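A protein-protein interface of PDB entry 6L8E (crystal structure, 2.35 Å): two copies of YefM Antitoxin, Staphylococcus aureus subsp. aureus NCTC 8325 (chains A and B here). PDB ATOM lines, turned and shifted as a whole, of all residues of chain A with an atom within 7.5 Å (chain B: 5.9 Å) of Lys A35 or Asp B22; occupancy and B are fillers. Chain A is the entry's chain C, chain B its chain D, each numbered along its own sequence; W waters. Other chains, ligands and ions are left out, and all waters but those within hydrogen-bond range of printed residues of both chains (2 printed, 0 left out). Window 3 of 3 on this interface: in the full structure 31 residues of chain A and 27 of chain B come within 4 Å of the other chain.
ND2 of Asn B21 sits at hydrogen-bond distance from O of Asn A36, at 3.0 Å.
ND2 of Asn B21 sits at hydrogen-bond distance from O of Lys A35, at 3.2 Å.
The side-chain carboxylate (OD2) of Asp A33 is in salt-bridge range of the side-chain amino group (NZ) of Lys B14.
The side-chain amino group (NZ) of Lys A35 is in salt-bridge range of the side-chain carboxylate (OD1) of Asp B22, at 3.3 Å.
OG of Ser A31 sits at hydrogen-bond distance from OD1 of Asp A33, at 2.7 Å.
The side-chain amide nitrogen (ND2) of Asn B21 lies within hydrogen-bond range of the backbone carbonyl oxygen (O) of Met B17.
O of Asp A34 sits close to OD1 of Asn A36 (3.5 Å).
The backbone NH of Lys A35 lies close to the side-chain carboxylate of Asp A33, at 3.3 Å.
N of Val A29 is in hydrogen-bond range of O of Val A37, at 2.8 Å.
The backbone NH of Ser A31 lies within hydrogen-bond range of the side-chain amide oxygen of Asn A36 (3.0 Å).
Met B17 touches Val A29 (CE to O, 3.5 Å).
Lys B14 touches Ser A31.
Met B17 touches Lys A35.
CD of Lys A35 touches CG2 of Thr B18 (3.8 Å).
CG1 of Val A37 touches CG of Met B17, at 3.8 Å.
Val A37 touches Val B20 (CG1 to CG2, 3.6 Å).
CG1 of Val A37 touches ND2 of Asn B21 (3.9 Å).
Lys A35 touches just these residues of chain B: Met B17, Thr B18, Asn B21 and Asp B22.
Printed residues of chain A within 4 Å of Asp B22: Lys A35 (3.3 Å).
Printed residues of chain B within 4 Å of Asp A33: Lys B14.
Printed residues of chain A within 4 Å of Thr B18: Lys A35.
The nearest printed residue of chain A that does not touch Asp B22 is Asn A36 (8.0 Å).
Of the 9 printed residues of chain B, 6 touch a printed residue of chain A.
Hydrophobic or aromatic side chains of chain B that line the printed part of chain A: Met B17 and Val B20.
Printed residues of chain A that touch a printed residue of chain B: Val A29, Ser A31, Asp A33, Lys A35, Asn A36 and Val A37.
Along chain A the printed residues that touch a printed residue of chain B span positions 29 to 37.
Among the printed residues, 11 pairs touch across the chains.
Among the printed residues, Asp or Glu carboxylates within 4 Å of a Lys or Arg side-chain nitrogen of the other chain: Asp A33 with Lys B14 (3.7 Å) and Lys A35 with Asp B22 (3.3 Å).
No position is printed for both chains.
Water W1 lies within hydrogen-bond range of OD1 of Asn B21 (2.8 Å) and O of Asn A36 (3.3 Å).
Water W2 bridges NZ of Lys B14 and N of Thr A32.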
ATOM      1  N   VAL A  29     -15.072  -3.848 -28.051  1.00  0.00           N
ATOM      2  CA  VAL A  29     -15.862  -2.649 -27.809  1.00  0.00           C
ATOM      3  C   VAL A  29     -16.565  -2.815 -26.470  1.00  0.00           C
ATOM      4  O   VAL A  29     -17.363  -3.743 -26.292  1.00  0.00           O
ATOM      5  CB  VAL A  29     -16.864  -2.394 -28.942  1.00  0.00           C
ATOM      6  CG1 VAL A  29     -17.602  -1.098 -28.694  1.00  0.00           C
ATOM      7  CG2 VAL A  29     -16.143  -2.357 -30.281  1.00  0.00           C
ATOM      8  N   THR A  30     -16.265  -1.922 -25.531  1.00  0.00           N
ATOM      9  CA  THR A  30     -16.783  -2.022 -24.177  1.00  0.00           C
ATOM     10  C   THR A  30     -18.098  -1.259 -24.044  1.00  0.00           C
ATOM     11  O   THR A  30     -18.410  -0.358 -24.827  1.00  0.00           O
ATOM     12  CB  THR A  30     -15.769  -1.493 -23.158  1.00  0.00           C
ATOM     13  OG1 THR A  30     -15.598  -0.080 -23.327  1.00  0.00           O
ATOM     14  CG2 THR A  30     -14.424  -2.187 -23.329  1.00  0.00           C
ATOM     15  N   SER A  31     -18.883  -1.660 -23.046  1.00  0.00           N
ATOM     16  CA  SER A  31     -20.092  -0.952 -22.653  1.00  0.00           C
ATOM     17  C   SER A  31     -20.144  -0.916 -21.134  1.00  0.00           C
ATOM     18  O   SER A  31     -19.502  -1.720 -20.453  1.00  0.00           O
ATOM     19  CB  SER A  31     -21.355  -1.609 -23.220  1.00  0.00           C
ATOM     20  OG  SER A  31     -21.654  -2.812 -22.537  1.00  0.00           O
ATOM     21  N   THR A  32     -20.919   0.030 -20.605  1.00  0.00           N
ATOM     22  CA  THR A  32     -20.957   0.234 -19.162  1.00  0.00           C
ATOM     23  C   THR A  32     -21.747  -0.837 -18.423  1.00  0.00           C
ATOM     24  O   THR A  32     -21.573  -0.978 -17.207  1.00  0.00           O
ATOM     25  CB  THR A  32     -21.530   1.613 -18.837  1.00  0.00           C
ATOM     26  OG1 THR A  32     -22.714   1.838 -19.613  1.00  0.00           O
ATOM     27  CG2 THR A  32     -20.504   2.694 -19.142  1.00  0.00           C
ATOM     28  N   ASP A  33     -22.603  -1.592 -19.109  1.00  0.00           N
ATOM     29  CA  ASP A  33     -23.310  -2.701 -18.485  1.00  0.00           C
ATOM     30  C   ASP A  33     -22.632  -4.040 -18.748  1.00  0.00           C
ATOM     31  O   ASP A  33     -23.267  -5.087 -18.584  1.00  0.00           O
ATOM     32  CB  ASP A  33     -24.765  -2.743 -18.953  1.00  0.00           C
ATOM     33  CG  ASP A  33     -24.893  -2.851 -20.456  1.00  0.00           C
ATOM     34  OD1 ASP A  33     -23.929  -3.283 -21.119  1.00  0.00           O
ATOM     35  OD2 ASP A  33     -25.965  -2.481 -20.980  1.00  0.00           O
ATOM     36  N   ASP A  34     -21.377  -4.023 -19.197  1.00  0.00           N
ATOM     37  CA  ASP A  34     -20.475  -5.166 -19.359  1.00  0.00           C
ATOM     38  C   ASP A  34     -20.776  -6.099 -20.537  1.00  0.00           C
ATOM     39  O   ASP A  34     -19.980  -7.024 -20.767  1.00  0.00           O
ATOM     40  CB  ASP A  34     -20.402  -6.036 -18.094  1.00  0.00           C
ATOM     41  CG  ASP A  34     -19.091  -5.877 -17.343  1.00  0.00           C
ATOM     42  OD1 ASP A  34     -18.011  -6.119 -17.927  1.00  0.00           O
ATOM     43  OD2 ASP A  34     -19.150  -5.513 -16.153  1.00  0.00           O
ATOM     44  N   LYS A  35     -21.872  -5.921 -21.281  1.00  0.00           N
ATOM     45  CA  LYS A  35     -22.080  -6.776 -22.451  1.00  0.00           C
ATOM     46  C   LYS A  35     -21.233  -6.227 -23.602  1.00  0.00           C
ATOM     47  O   LYS A  35     -21.701  -5.533 -24.513  1.00  0.00           O
ATOM     48  CB  LYS A  35     -23.563  -6.915 -22.800  1.00  0.00           C
ATOM     49  CG  LYS A  35     -24.408  -5.662 -22.868  1.00  0.00           C
ATOM     50  CD  LYS A  35     -25.875  -6.021 -22.634  1.00  0.00           C
ATOM     51  CE  LYS A  35     -25.997  -7.023 -21.492  1.00  0.00           C
ATOM     52  NZ  LYS A  35     -27.399  -7.374 -21.144  1.00  0.00           N
ATOM     53  N   ASN A  36     -19.944  -6.556 -23.541  1.00  0.00           N
ATOM     54  CA  ASN A  36     -18.957  -6.178 -24.536  1.00  0.00           C
ATOM     55  C   ASN A  36     -19.032  -7.099 -25.749  1.00  0.00           C
ATOM     56  O   ASN A  36     -19.597  -8.198 -25.703  1.00  0.00           O
ATOM     57  CB  ASN A  36     -17.545  -6.233 -23.947  1.00  0.00           C
ATOM     58  CG  ASN A  36     -17.403  -5.401 -22.688  1.00  0.00           C
ATOM     59  OD1 ASN A  36     -18.211  -4.512 -22.425  1.00  0.00           O
ATOM     60  ND2 ASN A  36     -16.370  -5.687 -21.902  1.00  0.00           N
ATOM     61  N   VAL A  37     -18.435  -6.633 -26.847  1.00  0.00           N
ATOM     62  CA  VAL A  37     -18.340  -7.398 -28.079  1.00  0.00           C
ATOM     63  C   VAL A  37     -16.900  -7.328 -28.564  1.00  0.00           C
ATOM     64  O   VAL A  37     -16.140  -6.430 -28.195  1.00  0.00           O
ATOM     65  CB  VAL A  37     -19.298  -6.879 -29.173  1.00  0.00           C
ATOM     66  CG1 VAL A  37     -20.726  -6.826 -28.660  1.00  0.00           C
ATOM     67  CG2 VAL A  37     -18.857  -5.504 -29.654  1.00  0.00           C
ATOM     68  N   LYS B  14     -25.846  -0.196 -30.158  1.00  0.00           N
ATOM     69  CA  LYS B  14     -26.051  -0.629 -28.777  1.00  0.00           C
ATOM     70  C   LYS B  14     -27.029  -1.795 -28.702  1.00  0.00           C
ATOM     71  O   LYS B  14     -26.814  -2.749 -27.944  1.00  0.00           O
ATOM     72  CB  LYS B  14     -26.543   0.540 -27.928  1.00  0.00           C
ATOM     73  CG  LYS B  14     -26.716   0.205 -26.454  1.00  0.00           C
ATOM     74  CD  LYS B  14     -25.378  -0.044 -25.760  1.00  0.00           C
ATOM     75  CE  LYS B  14     -25.565  -0.288 -24.265  1.00  0.00           C
ATOM     76  NZ  LYS B  14     -24.274  -0.388 -23.534  1.00  0.00           N
ATOM     77  N   MET B  17     -25.123  -4.862 -29.801  1.00  0.00           N
ATOM     78  CA  MET B  17     -24.213  -5.319 -28.753  1.00  0.00           C
ATOM     79  C   MET B  17     -24.962  -6.069 -27.662  1.00  0.00           C
ATOM     80  O   MET B  17     -24.499  -7.113 -27.183  1.00  0.00           O
ATOM     81  CB  MET B  17     -23.456  -4.133 -28.154  1.00  0.00           C
ATOM     82  CG  MET B  17     -22.452  -3.501 -29.097  1.00  0.00           C
ATOM     83  SD  MET B  17     -21.649  -2.062 -28.371  1.00  0.00           S
ATOM     84  CE  MET B  17     -20.612  -2.836 -27.137  1.00  0.00           C
ATOM     85  N   THR B  18     -26.116  -5.539 -27.251  1.00  0.00           N
ATOM     86  CA  THR B  18     -26.954  -6.227 -26.278  1.00  0.00           C
ATOM     87  C   THR B  18     -27.408  -7.578 -26.809  1.00  0.00           C
ATOM     88  O   THR B  18     -27.368  -8.584 -26.094  1.00  0.00           O
ATOM     89  CB  THR B  18     -28.166  -5.366 -25.922  1.00  0.00           C
ATOM     90  OG1 THR B  18     -27.727  -4.064 -25.518  1.00  0.00           O
ATOM     91  CG2 THR B  18     -28.954  -6.001 -24.787  1.00  0.00           C
ATOM     92  N   LYS B  19     -27.819  -7.623 -28.079  1.00  0.00           N
ATOM     93  CA  LYS B  19     -28.433  -8.834 -28.614  1.00  0.00           C
ATOM     94  C   LYS B  19     -27.433  -9.980 -28.713  1.00  0.00           C
ATOM     95  O   LYS B  19     -27.762 -11.124 -28.380  1.00  0.00           O
ATOM     96  CB  LYS B  19     -29.066  -8.555 -29.975  1.00  0.00           C
ATOM     97  CG  LYS B  19     -29.771  -9.764 -30.575  1.00  0.00           C
ATOM     98  CD  LYS B  19     -30.760  -9.352 -31.646  1.00  0.00           C
ATOM     99  CE  LYS B  19     -31.790 -10.444 -31.860  1.00  0.00           C
ATOM    100  NZ  LYS B  19     -32.567 -10.707 -30.613  1.00  0.00           N
ATOM    101  N   VAL B  20     -26.216  -9.705 -29.187  1.00  0.00           N
ATOM    102  CA  VAL B  20     -25.231 -10.776 -29.313  1.00  0.00           C
ATOM    103  C   VAL B  20     -24.788 -11.296 -27.954  1.00  0.00           C
ATOM    104  O   VAL B  20     -24.345 -12.445 -27.850  1.00  0.00           O
ATOM    105  CB  VAL B  20     -24.013 -10.324 -30.141  1.00  0.00           C
ATOM    106  CG1 VAL B  20     -24.448  -9.897 -31.529  1.00  0.00           C
ATOM    107  CG2 VAL B  20     -23.266  -9.202 -29.438  1.00  0.00           C
ATOM    108  N   ASN B  21     -24.893 -10.484 -26.900  1.00  0.00           N
ATOM    109  CA  ASN B  21     -24.609 -10.986 -25.559  1.00  0.00           C
ATOM    110  C   ASN B  21     -25.788 -11.782 -25.011  1.00  0.00           C
ATOM    111  O   ASN B  21     -25.603 -12.861 -24.437  1.00  0.00           O
ATOM    112  CB  ASN B  21     -24.260  -9.834 -24.619  1.00  0.00           C
ATOM    113  CG  ASN B  21     -22.815  -9.399 -24.740  1.00  0.00           C
ATOM    114  OD1 ASN B  21     -21.946  -9.892 -24.021  1.00  0.00           O
ATOM    115  ND2 ASN B  21     -22.555  -8.457 -25.637  1.00  0.00           N
ATOM    116  N   ASP B  22     -27.008 -11.265 -25.183  1.00  0.00           N
ATOM    117  CA  ASP B  22     -28.188 -11.952 -24.667  1.00  0.00           C
ATOM    118  C   ASP B  22     -28.417 -13.279 -25.380  1.00  0.00           C
ATOM    119  O   ASP B  22     -28.727 -14.288 -24.738  1.00  0.00           O
ATOM    120  CB  ASP B  22     -29.417 -11.055 -24.803  1.00  0.00           C
ATOM    121  CG  ASP B  22     -29.425  -9.921 -23.808  1.00  0.00           C
ATOM    122  OD1 ASP B  22     -28.620  -9.965 -22.848  1.00  0.00           O
ATOM    123  OD2 ASP B  22     -30.235  -8.988 -23.992  1.00  0.00           O
ATOM    124  N   ASP B  23     -28.257 -13.304 -26.701  1.00  0.00           N
ATOM    125  CA  ASP B  23     -28.623 -14.460 -27.507  1.00  0.00           C
ATOM    126  C   ASP B  23     -27.442 -15.355 -27.854  1.00  0.00           C
ATOM    127  O   ASP B  23     -27.649 -16.426 -28.437  1.00  0.00           O
ATOM    128  CB  ASP B  23     -29.302 -14.007 -28.801  1.00  0.00           C
ATOM    129  CG  ASP B  23     -30.584 -13.242 -28.552  1.00  0.00           C
ATOM    130  OD1 ASP B  23     -31.028 -13.168 -27.386  1.00  0.00           O
ATOM    131  OD2 ASP B  23     -31.150 -12.708 -29.525  1.00  0.00           O
ATOM    132  N   SER B  24     -26.218 -14.941 -27.524  1.00  0.00           N
ATOM    133  CA  SER B  24     -25.011 -15.698 -27.850  1.00  0.00           C
ATOM    134  C   SER B  24     -24.944 -16.054 -29.333  1.00  0.00           C
ATOM    135  O   SER B  24     -24.499 -17.140 -29.712  1.00  0.00           O
ATOM    136  CB  SER B  24     -24.898 -16.963 -26.995  1.00  0.00           C
ATOM    137  OG  SER B  24     -24.805 -16.639 -25.616  1.00  0.00           O
HETATM  138  O   HOH W   1     -19.362 -10.665 -23.477  1.00  0.00           O
HETATM  139  O   HOH W   2     -22.056   1.616 -23.008  1.00  0.00           O
